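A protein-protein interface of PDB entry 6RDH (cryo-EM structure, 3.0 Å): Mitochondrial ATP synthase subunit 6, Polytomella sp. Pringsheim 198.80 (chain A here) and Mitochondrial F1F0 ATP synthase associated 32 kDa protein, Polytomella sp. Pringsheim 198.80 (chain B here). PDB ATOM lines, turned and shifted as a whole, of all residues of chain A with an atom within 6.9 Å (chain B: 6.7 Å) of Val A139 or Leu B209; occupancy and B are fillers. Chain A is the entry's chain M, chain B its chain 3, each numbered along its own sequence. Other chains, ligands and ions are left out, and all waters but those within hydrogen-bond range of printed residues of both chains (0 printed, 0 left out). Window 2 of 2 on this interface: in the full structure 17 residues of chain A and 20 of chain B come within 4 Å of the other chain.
The side-chain carboxylate (OD2) of Asp A143 lies within salt-bridge range of the guanidinium group (NH2) of Arg B213, 2.5 Å away.
ND1 of His B207 sits close to N of Leu B209, 3.3 Å away.
The backbone carbonyl oxygen of Tyr B208 is in hydrogen-bond range of the guanidinium group of Arg B242 (3.1 Å).
CD1 of Leu A135 touches CE2 of Tyr B208 (3.7 Å).
CD1 of Leu A135 touches CD2 of Leu B209, at 3.8 Å.
Arg B242 touches Leu A135.
CG1 of Val B212 touches CA of Pro A136, 3.7 Å away.
CG of Pro A136 touches O of Arg B242, 3.2 Å away.
Val A139 touches Leu B209.
CG1 of Val A139 touches CG1 of Val B212, at 3.8 Å.
Val A139 touches Arg B213.
Printed residues of chain B within 4 Å of Val A139: Leu B209, Val B212 and Arg B213.
Of chain A, only Leu A135 (3.8 Å) and Val A139 (3.8 Å) come within 4 Å of Leu B209.
Of the printed residues of chain A, Tyr B208 touches Leu A135.
Printed residues of chain B within 4 Å of Pro A136: Val B212 and Arg B242.
Of the printed residues of chain B, Leu A135 touches Tyr B208, Leu B209 and Arg B242.
Leu A134 touches none of the printed residues of chain B.
Ser A142 touches none of the printed residues of chain B.
The nearest residue of chain A that does not touch Leu B209 is Pro A136 (6.1 Å).
Hydrophobic or aromatic side chains of chain A within 4 Å of the printed part of chain B: Leu A135, Pro A136 and Val A139.
Of the 11 printed residues of chain B, 5 touch a printed residue of chain A.
Among the printed residues, Asp or Glu carboxylates within 4 Å of a Lys or Arg side-chain nitrogen of the other chain: Asp A143 with Arg B213 (2.5 Å).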
ATOM      1  N   LEU A 134      17.383 -13.173   6.262  1.00  0.00           N
ATOM      2  CA  LEU A 134      18.719 -13.002   5.716  1.00  0.00           C
ATOM      3  C   LEU A 134      19.523 -11.911   6.405  1.00  0.00           C
ATOM      4  O   LEU A 134      20.716 -11.782   6.124  1.00  0.00           O
ATOM      5  CB  LEU A 134      18.630 -12.690   4.224  1.00  0.00           C
ATOM      6  CG  LEU A 134      19.761 -13.239   3.365  1.00  0.00           C
ATOM      7  CD1 LEU A 134      19.819 -14.738   3.475  1.00  0.00           C
ATOM      8  CD2 LEU A 134      19.573 -12.816   1.941  1.00  0.00           C
ATOM      9  N   LEU A 135      18.919 -11.137   7.294  1.00  0.00           N
ATOM     10  CA  LEU A 135      19.586 -10.020   7.956  1.00  0.00           C
ATOM     11  C   LEU A 135      20.792 -10.387   8.819  1.00  0.00           C
ATOM     12  O   LEU A 135      21.764  -9.626   8.797  1.00  0.00           O
ATOM     13  CB  LEU A 135      18.595  -9.228   8.804  1.00  0.00           C
ATOM     14  CG  LEU A 135      17.961  -8.007   8.160  1.00  0.00           C
ATOM     15  CD1 LEU A 135      17.120  -7.312   9.188  1.00  0.00           C
ATOM     16  CD2 LEU A 135      19.006  -7.085   7.588  1.00  0.00           C
ATOM     17  N   PRO A 136      20.815 -11.484   9.593  1.00  0.00           N
ATOM     18  CA  PRO A 136      22.082 -11.817  10.254  1.00  0.00           C
ATOM     19  C   PRO A 136      23.143 -12.298   9.302  1.00  0.00           C
ATOM     20  O   PRO A 136      24.325 -12.084   9.572  1.00  0.00           O
ATOM     21  CB  PRO A 136      21.693 -12.910  11.251  1.00  0.00           C
ATOM     22  CG  PRO A 136      20.292 -12.749  11.441  1.00  0.00           C
ATOM     23  CD  PRO A 136      19.746 -12.339  10.142  1.00  0.00           C
ATOM     24  N   ALA A 137      22.765 -12.916   8.188  1.00  0.00           N
ATOM     25  CA  ALA A 137      23.753 -13.280   7.185  1.00  0.00           C
ATOM     26  C   ALA A 137      24.331 -12.055   6.507  1.00  0.00           C
ATOM     27  O   ALA A 137      25.523 -12.028   6.203  1.00  0.00           O
ATOM     28  CB  ALA A 137      23.132 -14.208   6.152  1.00  0.00           C
ATOM     29  N   VAL A 138      23.513 -11.023   6.302  1.00  0.00           N
ATOM     30  CA  VAL A 138      23.983  -9.786   5.689  1.00  0.00           C
ATOM     31  C   VAL A 138      24.871  -9.012   6.655  1.00  0.00           C
ATOM     32  O   VAL A 138      25.920  -8.490   6.266  1.00  0.00           O
ATOM     33  CB  VAL A 138      22.776  -8.963   5.214  1.00  0.00           C
ATOM     34  CG1 VAL A 138      23.172  -7.557   4.866  1.00  0.00           C
ATOM     35  CG2 VAL A 138      22.166  -9.627   4.020  1.00  0.00           C
ATOM     36  N   VAL A 139      24.488  -8.961   7.932  1.00  0.00           N
ATOM     37  CA  VAL A 139      25.322  -8.334   8.954  1.00  0.00           C
ATOM     38  C   VAL A 139      26.636  -9.090   9.111  1.00  0.00           C
ATOM     39  O   VAL A 139      27.707  -8.487   9.235  1.00  0.00           O
ATOM     40  CB  VAL A 139      24.535  -8.251  10.275  1.00  0.00           C
ATOM     41  CG1 VAL A 139      25.428  -7.976  11.451  1.00  0.00           C
ATOM     42  CG2 VAL A 139      23.490  -7.186  10.177  1.00  0.00           C
ATOM     43  N   ASP A 140      26.586 -10.419   9.019  1.00  0.00           N
ATOM     44  CA  ASP A 140      27.786 -11.229   9.168  1.00  0.00           C
ATOM     45  C   ASP A 140      28.711 -11.093   7.971  1.00  0.00           C
ATOM     46  O   ASP A 140      29.934 -11.086   8.128  1.00  0.00           O
ATOM     47  CB  ASP A 140      27.392 -12.683   9.363  1.00  0.00           C
ATOM     48  CG  ASP A 140      28.567 -13.602   9.339  1.00  0.00           C
ATOM     49  OD1 ASP A 140      29.388 -13.536  10.275  1.00  0.00           O
ATOM     50  OD2 ASP A 140      28.674 -14.392   8.383  1.00  0.00           O
ATOM     51  N   ALA A 141      28.149 -10.986   6.768  1.00  0.00           N
ATOM     52  CA  ALA A 141      28.966 -10.708   5.595  1.00  0.00           C
ATOM     53  C   ALA A 141      29.539  -9.304   5.652  1.00  0.00           C
ATOM     54  O   ALA A 141      30.637  -9.059   5.153  1.00  0.00           O
ATOM     55  CB  ALA A 141      28.145 -10.895   4.326  1.00  0.00           C
ATOM     56  N   SER A 142      28.817  -8.371   6.264  1.00  0.00           N
ATOM     57  CA  SER A 142      29.337  -7.029   6.455  1.00  0.00           C
ATOM     58  C   SER A 142      30.362  -6.934   7.573  1.00  0.00           C
ATOM     59  O   SER A 142      31.012  -5.897   7.688  1.00  0.00           O
ATOM     60  CB  SER A 142      28.192  -6.068   6.731  1.00  0.00           C
ATOM     61  OG  SER A 142      28.678  -4.771   7.003  1.00  0.00           O
ATOM     62  N   ASP A 143      30.503  -7.953   8.418  1.00  0.00           N
ATOM     63  CA  ASP A 143      31.583  -7.966   9.397  1.00  0.00           C
ATOM     64  C   ASP A 143      32.727  -8.893   9.030  1.00  0.00           C
ATOM     65  O   ASP A 143      33.718  -8.936   9.759  1.00  0.00           O
ATOM     66  CB  ASP A 143      31.076  -8.352  10.785  1.00  0.00           C
ATOM     67  CG  ASP A 143      29.930  -7.498  11.242  1.00  0.00           C
ATOM     68  OD1 ASP A 143      30.024  -6.262  11.108  1.00  0.00           O
ATOM     69  OD2 ASP A 143      28.951  -8.050  11.780  1.00  0.00           O
ATOM     70  N   LYS A 144      32.610  -9.650   7.951  1.00  0.00           N
ATOM     71  CA  LYS A 144      33.731 -10.402   7.418  1.00  0.00           C
ATOM     72  C   LYS A 144      34.334  -9.731   6.200  1.00  0.00           C
ATOM     73  O   LYS A 144      35.259 -10.274   5.598  1.00  0.00           O
ATOM     74  CB  LYS A 144      33.303 -11.829   7.085  1.00  0.00           C
ATOM     75  CG  LYS A 144      32.904 -12.621   8.313  1.00  0.00           C
ATOM     76  CD  LYS A 144      32.698 -14.085   8.015  1.00  0.00           C
ATOM     77  CE  LYS A 144      31.672 -14.287   6.929  1.00  0.00           C
ATOM     78  NZ  LYS A 144      31.357 -15.724   6.758  1.00  0.00           N
ATOM     79  N   PHE A 315      29.284 -16.408   2.064  1.00  0.00           N
ATOM     80  CA  PHE A 315      27.981 -15.980   2.549  1.00  0.00           C
ATOM     81  C   PHE A 315      27.311 -17.150   3.246  1.00  0.00           C
ATOM     82  O   PHE A 315      27.133 -18.210   2.641  1.00  0.00           O
ATOM     83  CB  PHE A 315      27.125 -15.479   1.393  1.00  0.00           C
ATOM     84  CG  PHE A 315      25.889 -14.756   1.825  1.00  0.00           C
ATOM     85  CD1 PHE A 315      25.967 -13.496   2.378  1.00  0.00           C
ATOM     86  CD2 PHE A 315      24.651 -15.335   1.668  1.00  0.00           C
ATOM     87  CE1 PHE A 315      24.834 -12.834   2.772  1.00  0.00           C
ATOM     88  CE2 PHE A 315      23.518 -14.673   2.061  1.00  0.00           C
ATOM     89  CZ  PHE A 315      23.613 -13.422   2.613  1.00  0.00           C
ATOM     90  N   ASN B 206      16.369   0.685  21.132  1.00  0.00           N
ATOM     91  CA  ASN B 206      17.659   0.170  20.716  1.00  0.00           C
ATOM     92  C   ASN B 206      17.603  -0.163  19.240  1.00  0.00           C
ATOM     93  O   ASN B 206      16.538  -0.173  18.627  1.00  0.00           O
ATOM     94  CB  ASN B 206      18.058  -1.062  21.521  1.00  0.00           C
ATOM     95  CG  ASN B 206      18.267  -0.753  22.974  1.00  0.00           C
ATOM     96  OD1 ASN B 206      18.054  -1.590  23.834  1.00  0.00           O
ATOM     97  ND2 ASN B 206      18.675   0.456  23.259  1.00  0.00           N
ATOM     98  N   HIS B 207      18.769  -0.425  18.665  1.00  0.00           N
ATOM     99  CA  HIS B 207      18.836  -0.704  17.242  1.00  0.00           C
ATOM    100  C   HIS B 207      18.238  -2.067  16.950  1.00  0.00           C
ATOM    101  O   HIS B 207      18.316  -2.987  17.759  1.00  0.00           O
ATOM    102  CB  HIS B 207      20.273  -0.646  16.755  1.00  0.00           C
ATOM    103  CG  HIS B 207      20.395  -0.468  15.281  1.00  0.00           C
ATOM    104  ND1 HIS B 207      20.674  -1.508  14.428  1.00  0.00           N
ATOM    105  CD2 HIS B 207      20.256   0.624  14.504  1.00  0.00           C
ATOM    106  CE1 HIS B 207      20.708  -1.063  13.188  1.00  0.00           C
ATOM    107  NE2 HIS B 207      20.447   0.226  13.206  1.00  0.00           N
ATOM    108  N   TYR B 208      17.618  -2.188  15.786  1.00  0.00           N
ATOM    109  CA  TYR B 208      16.884  -3.398  15.466  1.00  0.00           C
ATOM    110  C   TYR B 208      17.783  -4.545  15.044  1.00  0.00           C
ATOM    111  O   TYR B 208      17.287  -5.656  14.848  1.00  0.00           O
ATOM    112  CB  TYR B 208      15.854  -3.100  14.387  1.00  0.00           C
ATOM    113  CG  TYR B 208      16.353  -3.094  12.973  1.00  0.00           C
ATOM    114  CD1 TYR B 208      17.198  -2.106  12.513  1.00  0.00           C
ATOM    115  CD2 TYR B 208      15.940  -4.058  12.084  1.00  0.00           C
ATOM    116  CE1 TYR B 208      17.632  -2.101  11.216  1.00  0.00           C
ATOM    117  CE2 TYR B 208      16.371  -4.059  10.797  1.00  0.00           C
ATOM    118  CZ  TYR B 208      17.211  -3.084  10.368  1.00  0.00           C
ATOM    119  OH  TYR B 208      17.621  -3.110   9.067  1.00  0.00           O
ATOM    120  N   LEU B 209      19.085  -4.314  14.911  1.00  0.00           N
ATOM    121  CA  LEU B 209      20.059  -5.366  14.693  1.00  0.00           C
ATOM    122  C   LEU B 209      20.907  -5.612  15.922  1.00  0.00           C
ATOM    123  O   LEU B 209      21.928  -6.287  15.829  1.00  0.00           O
ATOM    124  CB  LEU B 209      20.964  -5.026  13.521  1.00  0.00           C
ATOM    125  CG  LEU B 209      20.294  -4.706  12.205  1.00  0.00           C
ATOM    126  CD1 LEU B 209      21.355  -4.278  11.274  1.00  0.00           C
ATOM    127  CD2 LEU B 209      19.601  -5.917  11.679  1.00  0.00           C
ATOM    128  N   ALA B 210      20.547  -5.049  17.044  1.00  0.00           N
ATOM    129  CA  ALA B 210      21.216  -5.393  18.285  1.00  0.00           C
ATOM    130  C   ALA B 210      20.929  -6.815  18.768  1.00  0.00           C
ATOM    131  O   ALA B 210      21.772  -7.371  19.479  1.00  0.00           O
ATOM    132  CB  ALA B 210      20.863  -4.378  19.368  1.00  0.00           C
ATOM    133  N   PRO B 211      19.774  -7.439  18.475  1.00  0.00           N
ATOM    134  CA  PRO B 211      19.715  -8.896  18.635  1.00  0.00           C
ATOM    135  C   PRO B 211      20.661  -9.673  17.741  1.00  0.00           C
ATOM    136  O   PRO B 211      21.076 -10.772  18.117  1.00  0.00           O
ATOM    137  CB  PRO B 211      18.257  -9.205  18.299  1.00  0.00           C
ATOM    138  CG  PRO B 211      17.554  -8.079  18.811  1.00  0.00           C
ATOM    139  CD  PRO B 211      18.396  -6.899  18.502  1.00  0.00           C
ATOM    140  N   VAL B 212      21.009  -9.153  16.566  1.00  0.00           N
ATOM    141  CA  VAL B 212      21.930  -9.860  15.685  1.00  0.00           C
ATOM    142  C   VAL B 212      23.341  -9.871  16.272  1.00  0.00           C
ATOM    143  O   VAL B 212      24.102 -10.822  16.075  1.00  0.00           O
ATOM    144  CB  VAL B 212      21.866  -9.218  14.286  1.00  0.00           C
ATOM    145  CG1 VAL B 212      22.760  -9.914  13.327  1.00  0.00           C
ATOM    146  CG2 VAL B 212      20.455  -9.250  13.767  1.00  0.00           C
ATOM    147  N   ARG B 213      23.688  -8.858  17.056  1.00  0.00           N
ATOM    148  CA  ARG B 213      24.989  -8.756  17.696  1.00  0.00           C
ATOM    149  C   ARG B 213      25.033  -9.409  19.068  1.00  0.00           C
ATOM    150  O   ARG B 213      25.931  -9.099  19.855  1.00  0.00           O
ATOM    151  CB  ARG B 213      25.385  -7.288  17.836  1.00  0.00           C
ATOM    152  CG  ARG B 213      26.119  -6.728  16.659  1.00  0.00           C
ATOM    153  CD  ARG B 213      27.540  -7.214  16.630  1.00  0.00           C
ATOM    154  NE  ARG B 213      28.364  -6.360  15.795  1.00  0.00           N
ATOM    155  CZ  ARG B 213      28.447  -6.469  14.478  1.00  0.00           C
ATOM    156  NH1 ARG B 213      29.219  -5.643  13.793  1.00  0.00           N
ATOM    157  NH2 ARG B 213      27.766  -7.405  13.843  1.00  0.00           N
ATOM    158  N   ALA B 214      24.095 -10.293  19.383  1.00  0.00           N
ATOM    159  CA  ALA B 214      23.904 -10.712  20.765  1.00  0.00           C
ATOM    160  C   ALA B 214      24.443 -12.097  21.070  1.00  0.00           C
ATOM    161  O   ALA B 214      24.997 -12.315  22.150  1.00  0.00           O
ATOM    162  CB  ALA B 214      22.421 -10.673  21.121  1.00  0.00           C
ATOM    163  N   THR B 239      11.479  -8.975  17.314  1.00  0.00           N
ATOM    164  CA  THR B 239      12.810  -8.378  17.383  1.00  0.00           C
ATOM    165  C   THR B 239      13.852  -9.400  17.810  1.00  0.00           C
ATOM    166  O   THR B 239      14.934  -9.479  17.225  1.00  0.00           O
ATOM    167  CB  THR B 239      12.805  -7.197  18.348  1.00  0.00           C
ATOM    168  OG1 THR B 239      11.752  -6.301  17.989  1.00  0.00           O
ATOM    169  CG2 THR B 239      14.107  -6.457  18.272  1.00  0.00           C
ATOM    170  N   ARG B 242      15.027 -12.089  15.254  1.00  0.00           N
ATOM    171  CA  ARG B 242      16.075 -11.770  14.291  1.00  0.00           C
ATOM    172  C   ARG B 242      17.425 -12.298  14.734  1.00  0.00           C
ATOM    173  O   ARG B 242      18.231 -12.694  13.895  1.00  0.00           O
ATOM    174  CB  ARG B 242      16.171 -10.268  14.049  1.00  0.00           C
ATOM    175  CG  ARG B 242      15.266  -9.754  12.971  1.00  0.00           C
ATOM    176  CD  ARG B 242      15.558  -8.304  12.700  1.00  0.00           C
ATOM    177  NE  ARG B 242      15.049  -7.427  13.744  1.00  0.00           N
ATOM    178  CZ  ARG B 242      13.845  -6.874  13.711  1.00  0.00           C
ATOM    179  NH1 ARG B 242      13.444  -6.082  14.689  1.00  0.00           N
ATOM    180  NH2 ARG B 242      13.041  -7.116  12.691  1.00  0.00           N
